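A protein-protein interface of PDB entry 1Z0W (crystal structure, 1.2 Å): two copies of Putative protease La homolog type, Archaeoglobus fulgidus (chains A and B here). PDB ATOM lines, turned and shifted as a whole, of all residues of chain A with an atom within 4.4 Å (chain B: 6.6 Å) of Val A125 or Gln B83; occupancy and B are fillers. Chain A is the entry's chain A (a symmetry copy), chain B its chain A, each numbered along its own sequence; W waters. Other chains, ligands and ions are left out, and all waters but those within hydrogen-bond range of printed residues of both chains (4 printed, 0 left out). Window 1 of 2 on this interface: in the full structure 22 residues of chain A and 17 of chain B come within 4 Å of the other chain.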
ATOM      1  N   ASN A  62      32.406   3.194   5.937  1.00  0.00           N
ATOM      2  CA  ASN A  62      31.350   2.962   4.946  1.00  0.00           C
ATOM      3  C   ASN A  62      31.870   3.126   3.533  1.00  0.00           C
ATOM      4  O   ASN A  62      31.571   2.336   2.638  1.00  0.00           O
ATOM      5  CB  ASN A  62      30.129   3.858   5.204  1.00  0.00           C
ATOM      6  CG  ASN A  62      29.440   3.484   6.504  1.00  0.00           C
ATOM      7  OD1 ASN A  62      29.868   2.637   7.276  1.00  0.00           O
ATOM      8  ND2 ASN A  62      28.322   4.152   6.735  1.00  0.00           N
ATOM      9  N   ALA A  65      33.861   0.123   2.244  1.00  0.00           N
ATOM     10  CA  ALA A  65      33.112  -1.014   1.679  1.00  0.00           C
ATOM     11  C   ALA A  65      32.945  -0.833   0.185  1.00  0.00           C
ATOM     12  O   ALA A  65      33.189  -1.768  -0.583  1.00  0.00           O
ATOM     13  CB  ALA A  65      31.771  -1.145   2.389  1.00  0.00           C
ATOM     14  N   ILE A  66      32.523   0.369  -0.243  1.00  0.00           N
ATOM     15  CA  ILE A  66      32.250   0.597  -1.657  1.00  0.00           C
ATOM     16  C   ILE A  66      33.528   0.642  -2.463  1.00  0.00           C
ATOM     17  O   ILE A  66      33.570   0.162  -3.600  1.00  0.00           O
ATOM     18  CB  ILE A  66      31.359   1.821  -1.867  1.00  0.00           C
ATOM     19  CG1 ILE A  66      31.899   3.207  -1.644  1.00  0.00           C
ATOM     20  CG2 ILE A  66      30.063   1.627  -1.061  1.00  0.00           C
ATOM     21  CD1 ILE A  66      30.959   4.243  -2.266  1.00  0.00           C
ATOM     22  N   LEU A 123      26.388   8.580   4.080  1.00  0.00           N
ATOM     23  CA  LEU A 123      26.695   7.491   3.168  1.00  0.00           C
ATOM     24  C   LEU A 123      26.342   6.137   3.764  1.00  0.00           C
ATOM     25  O   LEU A 123      26.774   5.782   4.859  1.00  0.00           O
ATOM     26  CB  LEU A 123      28.179   7.474   2.851  1.00  0.00           C
ATOM     27  CG  LEU A 123      28.586   6.434   1.809  1.00  0.00           C
ATOM     28  CD1 LEU A 123      28.022   6.743   0.437  1.00  0.00           C
ATOM     29  CD2 LEU A 123      30.105   6.274   1.773  1.00  0.00           C
ATOM     30  N   SER A 124      25.542   5.371   3.050  1.00  0.00           N
ATOM     31  CA  SER A 124      25.316   3.969   3.430  1.00  0.00           C
ATOM     32  C   SER A 124      26.445   3.110   2.923  1.00  0.00           C
ATOM     33  O   SER A 124      27.131   3.392   1.952  1.00  0.00           O
ATOM     34  CB  SER A 124      23.975   3.483   2.952  1.00  0.00           C
ATOM     35  OG  SER A 124      24.043   2.857   1.729  1.00  0.00           O
ATOM     36  N   VAL A 125      26.610   1.950   3.588  1.00  0.00           N
ATOM     37  CA  VAL A 125      27.590   0.950   3.179  1.00  0.00           C
ATOM     38  C   VAL A 125      27.331   0.386   1.791  1.00  0.00           C
ATOM     39  O   VAL A 125      28.236  -0.213   1.222  1.00  0.00           O
ATOM     40  CB  VAL A 125      27.740  -0.190   4.194  1.00  0.00           C
ATOM     41  CG1 VAL A 125      28.342   0.295   5.496  1.00  0.00           C
ATOM     42  CG2 VAL A 125      26.400  -0.927   4.429  1.00  0.00           C
ATOM     43  N   LYS A 126      26.139   0.611   1.257  1.00  0.00           N
ATOM     44  CA  LYS A 126      25.774   0.185  -0.074  1.00  0.00           C
ATOM     45  C   LYS A 126      25.933   1.289  -1.115  1.00  0.00           C
ATOM     46  O   LYS A 126      25.737   1.084  -2.298  1.00  0.00           O
ATOM     47  CB  LYS A 126      24.320  -0.323  -0.097  1.00  0.00           C
ATOM     48  CG  LYS A 126      24.188  -1.641   0.668  1.00  0.00           C
ATOM     49  CD  LYS A 126      22.877  -2.305   0.430  1.00  0.00           C
ATOM     50  CE  LYS A 126      22.740  -2.911  -0.945  1.00  0.00           C
ATOM     51  NZ  LYS A 126      23.852  -3.793  -1.406  1.00  0.00           N
ATOM     52  N   GLY A 127      26.342   2.490  -0.679  1.00  0.00           N
ATOM     53  CA  GLY A 127      26.515   3.611  -1.587  1.00  0.00           C
ATOM     54  C   GLY A 127      25.377   4.590  -1.705  1.00  0.00           C
ATOM     55  O   GLY A 127      25.471   5.565  -2.435  1.00  0.00           O
ATOM     56  N   LEU A 130      21.782   8.899   2.335  1.00  0.00           N
ATOM     57  CA  LEU A 130      20.663   8.881   3.253  1.00  0.00           C
ATOM     58  C   LEU A 130      20.378  10.277   3.760  1.00  0.00           C
ATOM     59  O   LEU A 130      21.287  11.123   3.863  1.00  0.00           O
ATOM     60  CB  LEU A 130      20.986   7.942   4.424  1.00  0.00           C
ATOM     61  CG  LEU A 130      21.366   6.498   4.033  1.00  0.00           C
ATOM     62  CD1 LEU A 130      21.619   5.712   5.297  1.00  0.00           C
ATOM     63  CD2 LEU A 130      20.338   5.856   3.159  1.00  0.00           C
ATOM     64  N   GLY B  13      20.089  -6.107   1.777  1.00  0.00           N
ATOM     65  CA  GLY B  13      20.991  -5.740   2.840  1.00  0.00           C
ATOM     66  C   GLY B  13      20.435  -4.803   3.884  1.00  0.00           C
ATOM     67  O   GLY B  13      21.214  -4.352   4.724  1.00  0.00           O
ATOM     68  N   PRO B  30      17.060   0.557  11.897  1.00  0.00           N
ATOM     69  CA  PRO B  30      17.418  -0.093  10.637  1.00  0.00           C
ATOM     70  C   PRO B  30      18.894  -0.440  10.633  1.00  0.00           C
ATOM     71  O   PRO B  30      19.749   0.282  11.138  1.00  0.00           O
ATOM     72  CB  PRO B  30      17.074   0.927   9.565  1.00  0.00           C
ATOM     73  CG  PRO B  30      16.210   1.936  10.240  1.00  0.00           C
ATOM     74  CD  PRO B  30      16.675   1.966  11.667  1.00  0.00           C
ATOM     75  N   ILE B  31      19.190  -1.581  10.015  1.00  0.00           N
ATOM     76  CA  ILE B  31      20.532  -2.090   9.783  1.00  0.00           C
ATOM     77  C   ILE B  31      20.776  -2.136   8.296  1.00  0.00           C
ATOM     78  O   ILE B  31      19.895  -2.582   7.550  1.00  0.00           O
ATOM     79  CB  ILE B  31      20.729  -3.559  10.330  1.00  0.00           C
ATOM     80  CG1 ILE B  31      20.247  -3.720  11.732  1.00  0.00           C
ATOM     81  CG2 ILE B  31      22.172  -4.026  10.041  1.00  0.00           C
ATOM     82  CD1 ILE B  31      21.093  -2.894  12.698  1.00  0.00           C
ATOM     83  N   ILE B  32      21.930  -1.715   7.863  1.00  0.00           N
ATOM     84  CA  ILE B  32      22.375  -1.891   6.499  1.00  0.00           C
ATOM     85  C   ILE B  32      23.679  -2.692   6.557  1.00  0.00           C
ATOM     86  O   ILE B  32      24.591  -2.360   7.316  1.00  0.00           O
ATOM     87  CB  ILE B  32      22.559  -0.616   5.718  1.00  0.00           C
ATOM     88  CG1 ILE B  32      21.336   0.312   5.871  1.00  0.00           C
ATOM     89  CG2 ILE B  32      22.832  -0.894   4.249  1.00  0.00           C
ATOM     90  CD1 ILE B  32      21.465   1.654   5.225  1.00  0.00           C
ATOM     91  N   ALA B  33      23.781  -3.770   5.764  1.00  0.00           N
ATOM     92  CA  ALA B  33      24.987  -4.585   5.702  1.00  0.00           C
ATOM     93  C   ALA B  33      25.505  -4.619   4.263  1.00  0.00           C
ATOM     94  O   ALA B  33      24.753  -4.609   3.321  1.00  0.00           O
ATOM     95  CB  ALA B  33      24.717  -5.991   6.203  1.00  0.00           C
ATOM     96  N   GLU B  34      26.829  -4.723   4.187  1.00  0.00           N
ATOM     97  CA  GLU B  34      27.507  -5.003   2.915  1.00  0.00           C
ATOM     98  C   GLU B  34      28.618  -5.998   3.196  1.00  0.00           C
ATOM     99  O   GLU B  34      29.226  -6.000   4.247  1.00  0.00           O
ATOM    100  CB  GLU B  34      28.026  -3.721   2.277  1.00  0.00           C
ATOM    101  CG  GLU B  34      28.730  -3.943   0.923  1.00  0.00           C
ATOM    102  CD  GLU B  34      27.812  -4.568  -0.101  1.00  0.00           C
ATOM    103  OE1 GLU B  34      27.503  -5.784  -0.005  1.00  0.00           O
ATOM    104  OE2 GLU B  34      27.381  -3.842  -1.024  1.00  0.00           O
ATOM    105  N   ILE B  47      33.373  -5.098  10.392  1.00  0.00           N
ATOM    106  CA  ILE B  47      33.631  -3.668  10.410  1.00  0.00           C
ATOM    107  C   ILE B  47      32.365  -2.958  10.887  1.00  0.00           C
ATOM    108  O   ILE B  47      31.352  -2.939  10.186  1.00  0.00           O
ATOM    109  CB  ILE B  47      34.127  -3.161   9.071  1.00  0.00           C
ATOM    110  CG1 ILE B  47      35.407  -3.946   8.681  1.00  0.00           C
ATOM    111  CG2 ILE B  47      34.396  -1.671   9.008  1.00  0.00           C
ATOM    112  CD1 ILE B  47      35.935  -3.713   7.287  1.00  0.00           C
ATOM    113  N   ALA B  48      32.462  -2.429  12.098  1.00  0.00           N
ATOM    114  CA  ALA B  48      31.366  -1.763  12.746  1.00  0.00           C
ATOM    115  C   ALA B  48      31.950  -0.699  13.674  1.00  0.00           C
ATOM    116  O   ALA B  48      33.035  -0.865  14.159  1.00  0.00           O
ATOM    117  CB  ALA B  48      30.492  -2.746  13.513  1.00  0.00           C
ATOM    118  N   HIS B  81      30.522  -5.405   6.698  1.00  0.00           N
ATOM    119  CA  HIS B  81      30.264  -4.048   7.174  1.00  0.00           C
ATOM    120  C   HIS B  81      28.830  -3.931   7.689  1.00  0.00           C
ATOM    121  O   HIS B  81      27.905  -4.205   6.940  1.00  0.00           O
ATOM    122  CB  HIS B  81      30.481  -3.027   6.054  1.00  0.00           C
ATOM    123  CG  HIS B  81      31.862  -2.892   5.591  1.00  0.00           C
ATOM    124  ND1 HIS B  81      32.605  -1.726   5.841  1.00  0.00           N
ATOM    125  CD2 HIS B  81      32.720  -3.649   4.910  1.00  0.00           C
ATOM    126  CE1 HIS B  81      33.830  -1.877   5.319  1.00  0.00           C
ATOM    127  NE2 HIS B  81      33.924  -3.041   4.708  1.00  0.00           N
ATOM    128  N   ILE B  82      28.692  -3.526   8.945  1.00  0.00           N
ATOM    129  CA  ILE B  82      27.404  -3.316   9.580  1.00  0.00           C
ATOM    130  C   ILE B  82      27.210  -1.847   9.939  1.00  0.00           C
ATOM    131  O   ILE B  82      28.060  -1.293  10.661  1.00  0.00           O
ATOM    132  CB  ILE B  82      27.241  -4.168  10.829  1.00  0.00           C
ATOM    133  CG1 ILE B  82      27.507  -5.674  10.568  1.00  0.00           C
ATOM    134  CG2 ILE B  82      25.895  -3.944  11.526  1.00  0.00           C
ATOM    135  CD1 ILE B  82      26.628  -6.288   9.503  1.00  0.00           C
ATOM    136  N   GLN B  83      26.131  -1.269   9.459  1.00  0.00           N
ATOM    137  CA  GLN B  83      25.753   0.105   9.723  1.00  0.00           C
ATOM    138  C   GLN B  83      24.422   0.146  10.456  1.00  0.00           C
ATOM    139  O   GLN B  83      23.452  -0.495  10.038  1.00  0.00           O
ATOM    140  CB  GLN B  83      25.638   0.836   8.384  1.00  0.00           C
ATOM    141  CG  GLN B  83      25.038   2.223   8.478  1.00  0.00           C
ATOM    142  CD  GLN B  83      25.111   2.975   7.189  1.00  0.00           C
ATOM    143  OE1 GLN B  83      25.217   2.365   6.115  1.00  0.00           O
ATOM    144  NE2 GLN B  83      25.056   4.308   7.269  1.00  0.00           N
ATOM    145  N   PHE B  84      24.358   0.926  11.523  1.00  0.00           N
ATOM    146  CA  PHE B  84      23.130   1.201  12.269  1.00  0.00           C
ATOM    147  C   PHE B  84      22.662   2.574  11.817  1.00  0.00           C
ATOM    148  O   PHE B  84      23.428   3.547  11.834  1.00  0.00           O
ATOM    149  CB  PHE B  84      23.400   1.206  13.754  1.00  0.00           C
ATOM    150  CG  PHE B  84      23.884  -0.120  14.323  1.00  0.00           C
ATOM    151  CD1 PHE B  84      22.981  -1.080  14.760  1.00  0.00           C
ATOM    152  CD2 PHE B  84      25.217  -0.403  14.418  1.00  0.00           C
ATOM    153  CE1 PHE B  84      23.392  -2.305  15.241  1.00  0.00           C
ATOM    154  CE2 PHE B  84      25.657  -1.628  14.936  1.00  0.00           C
ATOM    155  CZ  PHE B  84      24.744  -2.594  15.368  1.00  0.00           C
ATOM    156  N   VAL B  85      21.454   2.655  11.367  1.00  0.00           N
ATOM    157  CA  VAL B  85      20.849   3.873  10.889  1.00  0.00           C
ATOM    158  C   VAL B  85      20.153   4.597  12.049  1.00  0.00           C
ATOM    159  O   VAL B  85      19.200   4.085  12.654  1.00  0.00           O
ATOM    160  CB  VAL B  85      19.891   3.647   9.720  1.00  0.00           C
ATOM    161  CG1 VAL B  85      19.347   4.975   9.205  1.00  0.00           C
ATOM    162  CG2 VAL B  85      20.541   2.901   8.566  1.00  0.00           C
HETATM  163  O   HOH W   1      28.358  -1.428  -1.537  1.00  0.00           O
HETATM  164  O   HOH W   2      23.860  -5.448   0.711  1.00  0.00           O
HETATM  165  O   HOH W   3      31.213   0.162   7.502  1.00  0.00           O
HETATM  166  O   HOH W   4      26.321  -1.529  -3.319  1.00  0.00           O
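ND2 of Asn A62 lies within hydrogen-bond range of O of Leu A123 (2.9 Å).
The side-chain hydroxyl (OG) of Ser A124 lies close to the backbone NH (N) of Lys A126 (3.1 Å).
The backbone carbonyl oxygen (O) of Ile B32 is in hydrogen-bond range of the backbone NH (N) of Gln B83 (2.9 Å).
OG of Ser A124 sits at hydrogen-bond distance from N of Gly A127 (3.3 Å).
O of Gly B13 is in hydrogen-bond range of N of Ala B33.
The backbone carbonyl oxygen (O) of Glu B34 lies within hydrogen-bond range of the backbone NH (N) of His B81 (2.8 Å).
NE2 of Gln B83 sits close to ND2 of Asn A62, 3.3 Å away.
The backbone carbonyl oxygen (O) of Leu A123 is in hydrogen-bond range of the side-chain amide nitrogen (NE2) of Gln B83, at 3.3 Å.
The side-chain carboxylate (OE2) of Glu B34 is in salt-bridge range of the side-chain amino group (NZ) of Lys A126.
N of Val A125 is in hydrogen-bond range of OE1 of Gln B83.
Of the 9 printed residues of chain A, 6 touch a printed residue of chain B.
Of the 13 printed residues of chain B, 5 touch a printed residue of chain A.
Printed residues of chain B that touch a printed residue of chain A: Ile B32, Ala B33, Glu B34, His B81 and Gln B83.
Hydrophobic or aromatic side chains of chain B that line the printed part of chain A: Ile B32 and His B81.
Among the printed residues, 12 pairs touch across the chains.
Among the printed residues, Asp or Glu carboxylates within 4 Å of a Lys or Arg side-chain nitrogen of the other chain: Lys A126 with Glu B34 (3.5 Å).
ND1 of His B81 touches CB of Ala A65, 3.6 Å away.
Ile B32 touches Ser A124 (CD1 to CB, 3.8 Å).
Ser A124 touches Gln B83.
CG2 of Ile B32 touches CG2 of Val A125 (3.6 Å).
Ala B33 touches Val A125 (C to CG2, 3.8 Å).
Glu B34 touches Val A125 (CB to O, 3.7 Å).
His B81 touches Val A125.
CG of Lys A126 touches CG2 of Ile B32, 3.9 Å away.
Printed residues of chain B within 4 Å of Val A125: Ile B32, Ala B33, Glu B34, His B81 and Gln B83.
Of the printed residues of chain B, Lys A126 touches Ile B32 and Glu B34.
Gly B13 touches none of the printed residues of chain A.
Of the printed residues of chain A, Glu B34 touches Val A125 (3.7 Å) and Lys A126 (3.5 Å).
Gln B83 touches just these residues of chain A: Asn A62, Leu A123, Ser A124 and Val A125.
Phe B84 touches none of the printed residues of chain A.
The nearest printed residue of chain B that does not touch Val A125 is Ile B82 (5.1 Å).
The nearest residue of chain A that does not touch Gln B83 is Leu A130 (4.2 Å).
Water W1 bridges the side-chain carboxylate of Glu B34 and the backbone carbonyl oxygen of Val A125.
Water W2 lies within hydrogen-bond range of the side-chain amino group (NZ) of Lys A126 and the backbone carbonyl oxygen (O) of Ala B33.
Water W3 bridges OD1 of Asn A62 (2.8 Å) and ND1 of His B81 (2.9 Å).
Water W4 bridges the backbone carbonyl oxygen of Lys A126 and the side-chain carboxylate of Glu B34.
No position is printed for both chains.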
